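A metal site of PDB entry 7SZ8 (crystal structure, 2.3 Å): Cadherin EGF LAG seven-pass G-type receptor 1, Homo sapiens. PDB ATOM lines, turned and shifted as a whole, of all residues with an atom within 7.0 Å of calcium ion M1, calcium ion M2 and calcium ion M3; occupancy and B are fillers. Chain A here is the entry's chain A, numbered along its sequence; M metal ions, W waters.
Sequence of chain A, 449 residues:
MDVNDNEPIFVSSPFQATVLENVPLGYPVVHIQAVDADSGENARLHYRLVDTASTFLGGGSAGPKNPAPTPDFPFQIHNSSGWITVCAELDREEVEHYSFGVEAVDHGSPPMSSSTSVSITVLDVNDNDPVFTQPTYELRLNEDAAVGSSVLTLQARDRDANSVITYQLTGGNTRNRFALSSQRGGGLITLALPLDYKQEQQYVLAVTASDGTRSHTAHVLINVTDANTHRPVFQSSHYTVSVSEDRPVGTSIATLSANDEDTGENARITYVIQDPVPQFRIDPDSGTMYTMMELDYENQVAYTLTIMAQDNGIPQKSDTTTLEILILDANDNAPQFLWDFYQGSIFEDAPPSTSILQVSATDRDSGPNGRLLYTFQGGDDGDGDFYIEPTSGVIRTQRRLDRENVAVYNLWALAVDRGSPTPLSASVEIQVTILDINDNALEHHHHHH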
ATOM      1  N   GLU A  21      22.574  -1.239 -19.178  1.00  0.00           N
ATOM      2  CA  GLU A  21      21.975  -2.593 -19.322  1.00  0.00           C
ATOM      3  C   GLU A  21      20.680  -2.695 -18.506  1.00  0.00           C
ATOM      4  O   GLU A  21      19.977  -3.681 -18.647  1.00  0.00           O
ATOM      5  CB  GLU A  21      22.962  -3.688 -18.933  1.00  0.00           C
ATOM      6  CG  GLU A  21      23.277  -3.798 -17.433  1.00  0.00           C
ATOM      7  CD  GLU A  21      24.114  -5.031 -17.143  1.00  0.00           C
ATOM      8  OE1 GLU A  21      23.830  -6.135 -17.710  1.00  0.00           O
ATOM      9  OE2 GLU A  21      25.116  -4.884 -16.426  1.00  0.00           O
ATOM     10  N   LEU A  90      17.867  -5.674 -21.287  1.00  0.00           N
ATOM     11  CA  LEU A  90      19.257  -5.743 -21.810  1.00  0.00           C
ATOM     12  C   LEU A  90      20.109  -6.510 -20.790  1.00  0.00           C
ATOM     13  O   LEU A  90      19.657  -6.648 -19.632  1.00  0.00           O
ATOM     14  CB  LEU A  90      19.778  -4.322 -21.968  1.00  0.00           C
ATOM     15  CG  LEU A  90      19.068  -3.448 -22.987  1.00  0.00           C
ATOM     16  CD1 LEU A  90      19.864  -2.163 -23.200  1.00  0.00           C
ATOM     17  CD2 LEU A  90      18.872  -4.190 -24.282  1.00  0.00           C
ATOM     18  N   ASP A  91      21.292  -6.988 -21.193  1.00  0.00           N
ATOM     19  CA  ASP A  91      22.233  -7.682 -20.282  1.00  0.00           C
ATOM     20  C   ASP A  91      23.635  -7.592 -20.868  1.00  0.00           C
ATOM     21  O   ASP A  91      23.922  -8.326 -21.780  1.00  0.00           O
ATOM     22  CB  ASP A  91      21.770  -9.128 -20.050  1.00  0.00           C
ATOM     23  CG  ASP A  91      22.663  -9.957 -19.129  1.00  0.00           C
ATOM     24  OD1 ASP A  91      23.553  -9.401 -18.504  1.00  0.00           O
ATOM     25  OD2 ASP A  91      22.415 -11.149 -19.029  1.00  0.00           O
ATOM     26  N   ARG A  92      24.491  -6.727 -20.328  1.00  0.00           N
ATOM     27  CA  ARG A  92      25.851  -6.530 -20.887  1.00  0.00           C
ATOM     28  C   ARG A  92      26.639  -7.849 -20.810  1.00  0.00           C
ATOM     29  O   ARG A  92      27.456  -8.083 -21.680  1.00  0.00           O
ATOM     30  CB  ARG A  92      26.621  -5.419 -20.153  1.00  0.00           C
ATOM     31  CG  ARG A  92      27.861  -5.005 -20.936  1.00  0.00           C
ATOM     32  CD  ARG A  92      29.007  -4.560 -20.079  1.00  0.00           C
ATOM     33  NE  ARG A  92      29.283  -5.558 -19.055  1.00  0.00           N
ATOM     34  CZ  ARG A  92      30.236  -6.459 -19.091  1.00  0.00           C
ATOM     35  NH1 ARG A  92      31.050  -6.549 -20.137  1.00  0.00           N
ATOM     36  NH2 ARG A  92      30.334  -7.296 -18.069  1.00  0.00           N
ATOM     37  N   GLU A  93      26.324  -8.694 -19.835  1.00  0.00           N
ATOM     38  CA  GLU A  93      27.003  -9.997 -19.634  1.00  0.00           C
ATOM     39  C   GLU A  93      26.538 -11.029 -20.676  1.00  0.00           C
ATOM     40  O   GLU A  93      27.182 -12.063 -20.761  1.00  0.00           O
ATOM     41  CB  GLU A  93      26.801 -10.501 -18.209  1.00  0.00           C
ATOM     42  CG  GLU A  93      27.620  -9.729 -17.206  1.00  0.00           C
ATOM     43  CD  GLU A  93      27.008  -8.390 -16.793  1.00  0.00           C
ATOM     44  OE1 GLU A  93      25.788  -8.354 -16.492  1.00  0.00           O
ATOM     45  OE2 GLU A  93      27.769  -7.385 -16.758  1.00  0.00           O
ATOM     46  N   GLU A  94      25.505 -10.718 -21.469  1.00  0.00           N
ATOM     47  CA  GLU A  94      25.053 -11.542 -22.618  1.00  0.00           C
ATOM     48  C   GLU A  94      25.614 -10.966 -23.922  1.00  0.00           C
ATOM     49  O   GLU A  94      26.138 -11.715 -24.706  1.00  0.00           O
ATOM     50  CB  GLU A  94      23.525 -11.567 -22.704  1.00  0.00           C
ATOM     51  CG  GLU A  94      22.988 -12.639 -23.656  1.00  0.00           C
ATOM     52  CD  GLU A  94      23.000 -14.051 -23.085  1.00  0.00           C
ATOM     53  OE1 GLU A  94      23.349 -14.987 -23.836  1.00  0.00           O
ATOM     54  OE2 GLU A  94      22.636 -14.218 -21.909  1.00  0.00           O
ATOM     55  N   LEU A 123      26.090  -0.463 -21.623  1.00  0.00           N
ATOM     56  CA  LEU A 123      26.975   0.001 -20.505  1.00  0.00           C
ATOM     57  C   LEU A 123      26.752  -0.868 -19.275  1.00  0.00           C
ATOM     58  O   LEU A 123      25.550  -1.248 -19.010  1.00  0.00           O
ATOM     59  CB  LEU A 123      26.699   1.484 -20.221  1.00  0.00           C
ATOM     60  CG  LEU A 123      27.134   2.439 -21.338  1.00  0.00           C
ATOM     61  CD1 LEU A 123      26.874   3.883 -20.966  1.00  0.00           C
ATOM     62  CD2 LEU A 123      28.600   2.229 -21.714  1.00  0.00           C
ATOM     63  N   ASP A 124      27.831  -1.184 -18.564  1.00  0.00           N
ATOM     64  CA  ASP A 124      27.860  -2.130 -17.424  1.00  0.00           C
ATOM     65  C   ASP A 124      27.276  -1.460 -16.193  1.00  0.00           C
ATOM     66  O   ASP A 124      27.619  -0.301 -15.956  1.00  0.00           O
ATOM     67  CB  ASP A 124      29.252  -2.573 -16.991  1.00  0.00           C
ATOM     68  CG  ASP A 124      29.266  -3.755 -16.027  1.00  0.00           C
ATOM     69  OD1 ASP A 124      28.639  -4.778 -16.380  1.00  0.00           O
ATOM     70  OD2 ASP A 124      29.969  -3.676 -14.967  1.00  0.00           O
ATOM     71  N   VAL A 125      26.419  -2.212 -15.481  1.00  0.00           N
ATOM     72  CA  VAL A 125      25.899  -1.948 -14.105  1.00  0.00           C
ATOM     73  C   VAL A 125      26.375  -3.117 -13.211  1.00  0.00           C
ATOM     74  O   VAL A 125      26.701  -4.234 -13.737  1.00  0.00           O
ATOM     75  CB  VAL A 125      24.362  -1.863 -14.160  1.00  0.00           C
ATOM     76  CG1 VAL A 125      23.716  -2.108 -12.819  1.00  0.00           C
ATOM     77  CG2 VAL A 125      23.880  -0.559 -14.770  1.00  0.00           C
ATOM     78  N   ASN A 126      26.445  -2.898 -11.900  1.00  0.00           N
ATOM     79  CA  ASN A 126      26.922  -3.912 -10.931  1.00  0.00           C
ATOM     80  C   ASN A 126      25.729  -4.786 -10.493  1.00  0.00           C
ATOM     81  O   ASN A 126      25.091  -4.474  -9.471  1.00  0.00           O
ATOM     82  CB  ASN A 126      27.659  -3.256  -9.753  1.00  0.00           C
ATOM     83  CG  ASN A 126      28.306  -4.316  -8.901  1.00  0.00           C
ATOM     84  OD1 ASN A 126      28.504  -5.437  -9.338  1.00  0.00           O
ATOM     85  ND2 ASN A 126      28.679  -3.961  -7.681  1.00  0.00           N
ATOM     86  N   ASP A 127      25.425  -5.813 -11.280  1.00  0.00           N
ATOM     87  CA  ASP A 127      24.211  -6.654 -11.114  1.00  0.00           C
ATOM     88  C   ASP A 127      24.669  -8.102 -10.912  1.00  0.00           C
ATOM     89  O   ASP A 127      23.784  -8.961 -10.849  1.00  0.00           O
ATOM     90  CB  ASP A 127      23.173  -6.416 -12.241  1.00  0.00           C
ATOM     91  CG  ASP A 127      23.636  -6.687 -13.670  1.00  0.00           C
ATOM     92  OD1 ASP A 127      24.831  -6.926 -13.861  1.00  0.00           O
ATOM     93  OD2 ASP A 127      22.756  -6.699 -14.616  1.00  0.00           O
ATOM     94  N   ASN A 128      25.972  -8.363 -10.737  1.00  0.00           N
ATOM     95  CA  ASN A 128      26.447  -9.725 -10.406  1.00  0.00           C
ATOM     96  C   ASN A 128      27.305  -9.713  -9.139  1.00  0.00           C
ATOM     97  O   ASN A 128      28.208  -8.831  -9.032  1.00  0.00           O
ATOM     98  CB  ASN A 128      27.244 -10.372 -11.536  1.00  0.00           C
ATOM     99  CG  ASN A 128      26.351 -10.730 -12.705  1.00  0.00           C
ATOM    100  OD1 ASN A 128      25.950 -11.877 -12.856  1.00  0.00           O
ATOM    101  ND2 ASN A 128      26.048  -9.752 -13.540  1.00  0.00           N
ATOM    102  N   ASP A 129      27.036 -10.685  -8.260  1.00  0.00           N
ATOM    103  CA  ASP A 129      27.860 -11.031  -7.076  1.00  0.00           C
ATOM    104  C   ASP A 129      29.182 -11.658  -7.552  1.00  0.00           C
ATOM    105  O   ASP A 129      29.188 -12.413  -8.531  1.00  0.00           O
ATOM    106  CB  ASP A 129      27.156 -12.007  -6.125  1.00  0.00           C
ATOM    107  CG  ASP A 129      25.857 -11.519  -5.497  1.00  0.00           C
ATOM    108  OD1 ASP A 129      25.484 -10.330  -5.679  1.00  0.00           O
ATOM    109  OD2 ASP A 129      25.187 -12.339  -4.836  1.00  0.00           O
ATOM    110  N   PRO A 130      30.314 -11.438  -6.852  1.00  0.00           N
ATOM    111  CA  PRO A 130      31.520 -12.256  -7.051  1.00  0.00           C
ATOM    112  C   PRO A 130      31.227 -13.709  -6.681  1.00  0.00           C
ATOM    113  O   PRO A 130      30.455 -13.944  -5.751  1.00  0.00           O
ATOM    114  CB  PRO A 130      32.570 -11.685  -6.075  1.00  0.00           C
ATOM    115  CG  PRO A 130      32.032 -10.302  -5.722  1.00  0.00           C
ATOM    116  CD  PRO A 130      30.518 -10.457  -5.784  1.00  0.00           C
ATOM    117  N   ASP A 158      34.007 -11.995 -11.109  1.00  0.00           N
ATOM    118  CA  ASP A 158      32.825 -11.111 -11.242  1.00  0.00           C
ATOM    119  C   ASP A 158      32.632 -10.925 -12.738  1.00  0.00           C
ATOM    120  O   ASP A 158      33.566 -10.401 -13.391  1.00  0.00           O
ATOM    121  CB  ASP A 158      33.042  -9.775 -10.533  1.00  0.00           C
ATOM    122  CG  ASP A 158      31.754  -9.074 -10.106  1.00  0.00           C
ATOM    123  OD1 ASP A 158      30.830  -8.979 -10.917  1.00  0.00           O
ATOM    124  OD2 ASP A 158      31.702  -8.584  -8.940  1.00  0.00           O
ATOM    125  N   ARG A 159      31.463 -11.330 -13.253  1.00  0.00           N
ATOM    126  CA  ARG A 159      31.091 -11.200 -14.678  1.00  0.00           C
ATOM    127  C   ARG A 159      30.902  -9.743 -15.072  1.00  0.00           C
ATOM    128  O   ARG A 159      30.852  -9.478 -16.230  1.00  0.00           O
ATOM    129  CB  ARG A 159      29.815 -11.992 -14.951  1.00  0.00           C
ATOM    130  CG  ARG A 159      30.002 -13.500 -14.830  1.00  0.00           C
ATOM    131  CD  ARG A 159      28.677 -14.236 -14.740  1.00  0.00           C
ATOM    132  NE  ARG A 159      27.944 -14.222 -15.997  1.00  0.00           N
ATOM    133  CZ  ARG A 159      26.697 -13.740 -16.169  1.00  0.00           C
ATOM    134  NH1 ARG A 159      25.996 -13.201 -15.180  1.00  0.00           N
ATOM    135  NH2 ARG A 159      26.148 -13.851 -17.369  1.00  0.00           N
ATOM    136  N   ASP A 160      30.774  -8.802 -14.133  1.00  0.00           N
ATOM    137  CA  ASP A 160      30.775  -7.356 -14.454  1.00  0.00           C
ATOM    138  C   ASP A 160      32.196  -6.977 -14.931  1.00  0.00           C
ATOM    139  O   ASP A 160      33.178  -7.425 -14.337  1.00  0.00           O
ATOM    140  CB  ASP A 160      30.155  -6.603 -13.277  1.00  0.00           C
ATOM    141  CG  ASP A 160      28.713  -7.000 -12.904  1.00  0.00           C
ATOM    142  OD1 ASP A 160      27.846  -7.001 -13.822  1.00  0.00           O
ATOM    143  OD2 ASP A 160      28.454  -7.275 -11.698  1.00  0.00           O
ATOM    144  N   ALA A 161      32.366  -6.166 -15.977  1.00  0.00           N
ATOM    145  CA  ALA A 161      33.691  -5.656 -16.430  1.00  0.00           C
ATOM    146  C   ALA A 161      34.259  -4.655 -15.397  1.00  0.00           C
ATOM    147  O   ALA A 161      35.459  -4.604 -15.219  1.00  0.00           O
ATOM    148  CB  ALA A 161      33.569  -5.007 -17.788  1.00  0.00           C
ATOM    149  N   ASN A 162      33.407  -3.947 -14.672  1.00  0.00           N
ATOM    150  CA  ASN A 162      33.816  -2.770 -13.852  1.00  0.00           C
ATOM    151  C   ASN A 162      33.865  -3.156 -12.366  1.00  0.00           C
ATOM    152  O   ASN A 162      33.720  -2.243 -11.504  1.00  0.00           O
ATOM    153  CB  ASN A 162      32.885  -1.580 -14.101  1.00  0.00           C
ATOM    154  CG  ASN A 162      32.795  -1.207 -15.572  1.00  0.00           C
ATOM    155  OD1 ASN A 162      33.766  -1.304 -16.328  1.00  0.00           O
ATOM    156  ND2 ASN A 162      31.635  -0.746 -15.969  1.00  0.00           N
ATOM    157  N   SER A 163      34.132  -4.420 -12.078  1.00  0.00           N
ATOM    158  CA  SER A 163      34.130  -4.997 -10.707  1.00  0.00           C
ATOM    159  C   SER A 163      35.546  -5.472 -10.396  1.00  0.00           C
ATOM    160  O   SER A 163      35.976  -6.380 -11.068  1.00  0.00           O
ATOM    161  CB  SER A 163      33.059  -6.091 -10.577  1.00  0.00           C
ATOM    162  OG  SER A 163      31.725  -5.547 -10.471  1.00  0.00           O
ATOM    163  N   VAL A 164      36.241  -4.765  -9.478  1.00  0.00           N
ATOM    164  CA  VAL A 164      37.493  -5.104  -8.738  1.00  0.00           C
ATOM    165  C   VAL A 164      37.132  -5.930  -7.501  1.00  0.00           C
ATOM    166  O   VAL A 164      36.264  -5.469  -6.708  1.00  0.00           O
ATOM    167  CB  VAL A 164      38.220  -3.832  -8.239  1.00  0.00           C
ATOM    168  CG1 VAL A 164      39.634  -4.137  -7.797  1.00  0.00           C
ATOM    169  CG2 VAL A 164      38.182  -2.669  -9.230  1.00  0.00           C
ATOM    170  N   ASP A 211      33.057  -6.760  -4.466  1.00  0.00           N
ATOM    171  CA  ASP A 211      33.305  -5.819  -5.576  1.00  0.00           C
ATOM    172  C   ASP A 211      33.178  -4.374  -5.044  1.00  0.00           C
ATOM    173  O   ASP A 211      33.242  -3.447  -5.845  1.00  0.00           O
ATOM    174  CB  ASP A 211      32.368  -6.082  -6.738  1.00  0.00           C
ATOM    175  CG  ASP A 211      30.896  -5.923  -6.419  1.00  0.00           C
ATOM    176  OD1 ASP A 211      30.602  -5.235  -5.426  1.00  0.00           O
ATOM    177  OD2 ASP A 211      30.052  -6.485  -7.180  1.00  0.00           O
ATOM    178  N   THR A 213      30.447  -3.445  -3.303  1.00  0.00           N
ATOM    179  CA  THR A 213      29.019  -3.314  -2.896  1.00  0.00           C
ATOM    180  C   THR A 213      28.386  -4.709  -2.697  1.00  0.00           C
ATOM    181  O   THR A 213      27.643  -4.836  -1.744  1.00  0.00           O
ATOM    182  CB  THR A 213      28.230  -2.362  -3.805  1.00  0.00           C
ATOM    183  OG1 THR A 213      27.767  -3.043  -4.959  1.00  0.00           O
ATOM    184  CG2 THR A 213      29.011  -1.189  -4.330  1.00  0.00           C
ATOM    185  N   ARG A 214      28.683  -5.693  -3.560  1.00  0.00           N
ATOM    186  CA  ARG A 214      28.160  -7.081  -3.493  1.00  0.00           C
ATOM    187  C   ARG A 214      29.253  -8.049  -3.063  1.00  0.00           C
ATOM    188  O   ARG A 214      30.463  -7.862  -3.487  1.00  0.00           O
ATOM    189  CB  ARG A 214      27.699  -7.563  -4.860  1.00  0.00           C
ATOM    190  CG  ARG A 214      26.564  -6.733  -5.426  1.00  0.00           C
ATOM    191  CD  ARG A 214      26.449  -7.030  -6.890  1.00  0.00           C
ATOM    192  NE  ARG A 214      25.162  -6.535  -7.313  1.00  0.00           N
ATOM    193  CZ  ARG A 214      24.039  -7.211  -7.246  1.00  0.00           C
ATOM    194  NH1 ARG A 214      24.008  -8.449  -6.784  1.00  0.00           N
ATOM    195  NH2 ARG A 214      22.954  -6.625  -7.712  1.00  0.00           N
HETATM  196 CA    CA M   1      29.863  -7.245  -9.510  1.00  0.00          CA
HETATM  197 CA    CA M   2      26.700  -6.079 -15.223  1.00  0.00          CA
HETATM  198 CA    CA M   3      23.498  -7.947 -16.582  1.00  0.00          CA
HETATM  199  O   HOH W   1      23.313  -9.935 -15.143  1.00  0.00           O
HETATM  200  O   HOH W   2      21.016  -8.076 -16.677  1.00  0.00           O
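Calcium ion M2 is bound by the side-chain carboxylate (OD1) of Asp 160, the side-chain carboxylate (OE2) of Glu 93, the side-chain carboxylate (OE2) of Glu 21, the backbone carbonyl oxygen (O) of Val 125, the side-chain carboxylate (OD1) of Asp 127, the side-chain carboxylate (OD1) of Asp 124 and the side-chain carboxylate (OE1) of Glu 93.
Of the 24 residues printed, 6 come within 4 Å of calcium ion M1.
Six residues have an atom within 4 Å of calcium ion M2: Glu 21, Glu 93, Asp 124, Val 125, Asp 127 and Asp 160. Along chain A the residues within 4 Å of calcium ion M2 span positions 21 to 160. The nearest printed residue that does not touch calcium ion M2 is Asn 128 (4.1 Å).
The backbone carbonyl oxygen of Leu 123 lies within hydrogen-bond range of the backbone NH of Glu 21 (3.0 Å). ND2 of Asn 126 is in hydrogen-bond range of OG1 of Thr 213, 3.0 Å away. OE2 of Glu 93 lies close to NH2 of Arg 92 (2.9 Å). OD1 of Asp 127 sits close to ND2 of Asn 128 (3.1 Å). The side-chain amide oxygen of Asn 128 is in hydrogen-bond range of the guanidinium group of Arg 159 (2.7 Å). The side-chain carboxylate of Asp 211 sits at hydrogen-bond distance from the backbone NH of Arg 214 (2.7 Å). NE of Arg 92 sits close to OD1 of Asp 124 (2.9 Å). The side-chain carboxylate (OD2) of Asp 124 sits at hydrogen-bond distance from the backbone NH (N) of Asn 162, 3.5 Å away.
Calcium ion M3 is bound by the side-chain carboxylate (OE1) of Glu 21, the side-chain carboxylate (OE1) of Glu 93, the side-chain carboxylate (OD1) of Asp 91, the side-chain carboxylate (OD2) of Asp 127, water W1 and water W2. Calcium ion M3 has six donor atoms within binding distance.
Calcium ion M1 is bound by OD1 of Asn 126 (2.3 Å), O of Asn 128 (2.3 Å), OD2 of Asp 158 (2.3 Å), OD1 of Asp 158 (2.4 Å), OD2 of Asp 211 (2.5 Å), OD2 of Asp 160 (2.6 Å) and OG of Ser 163 (2.7 Å).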
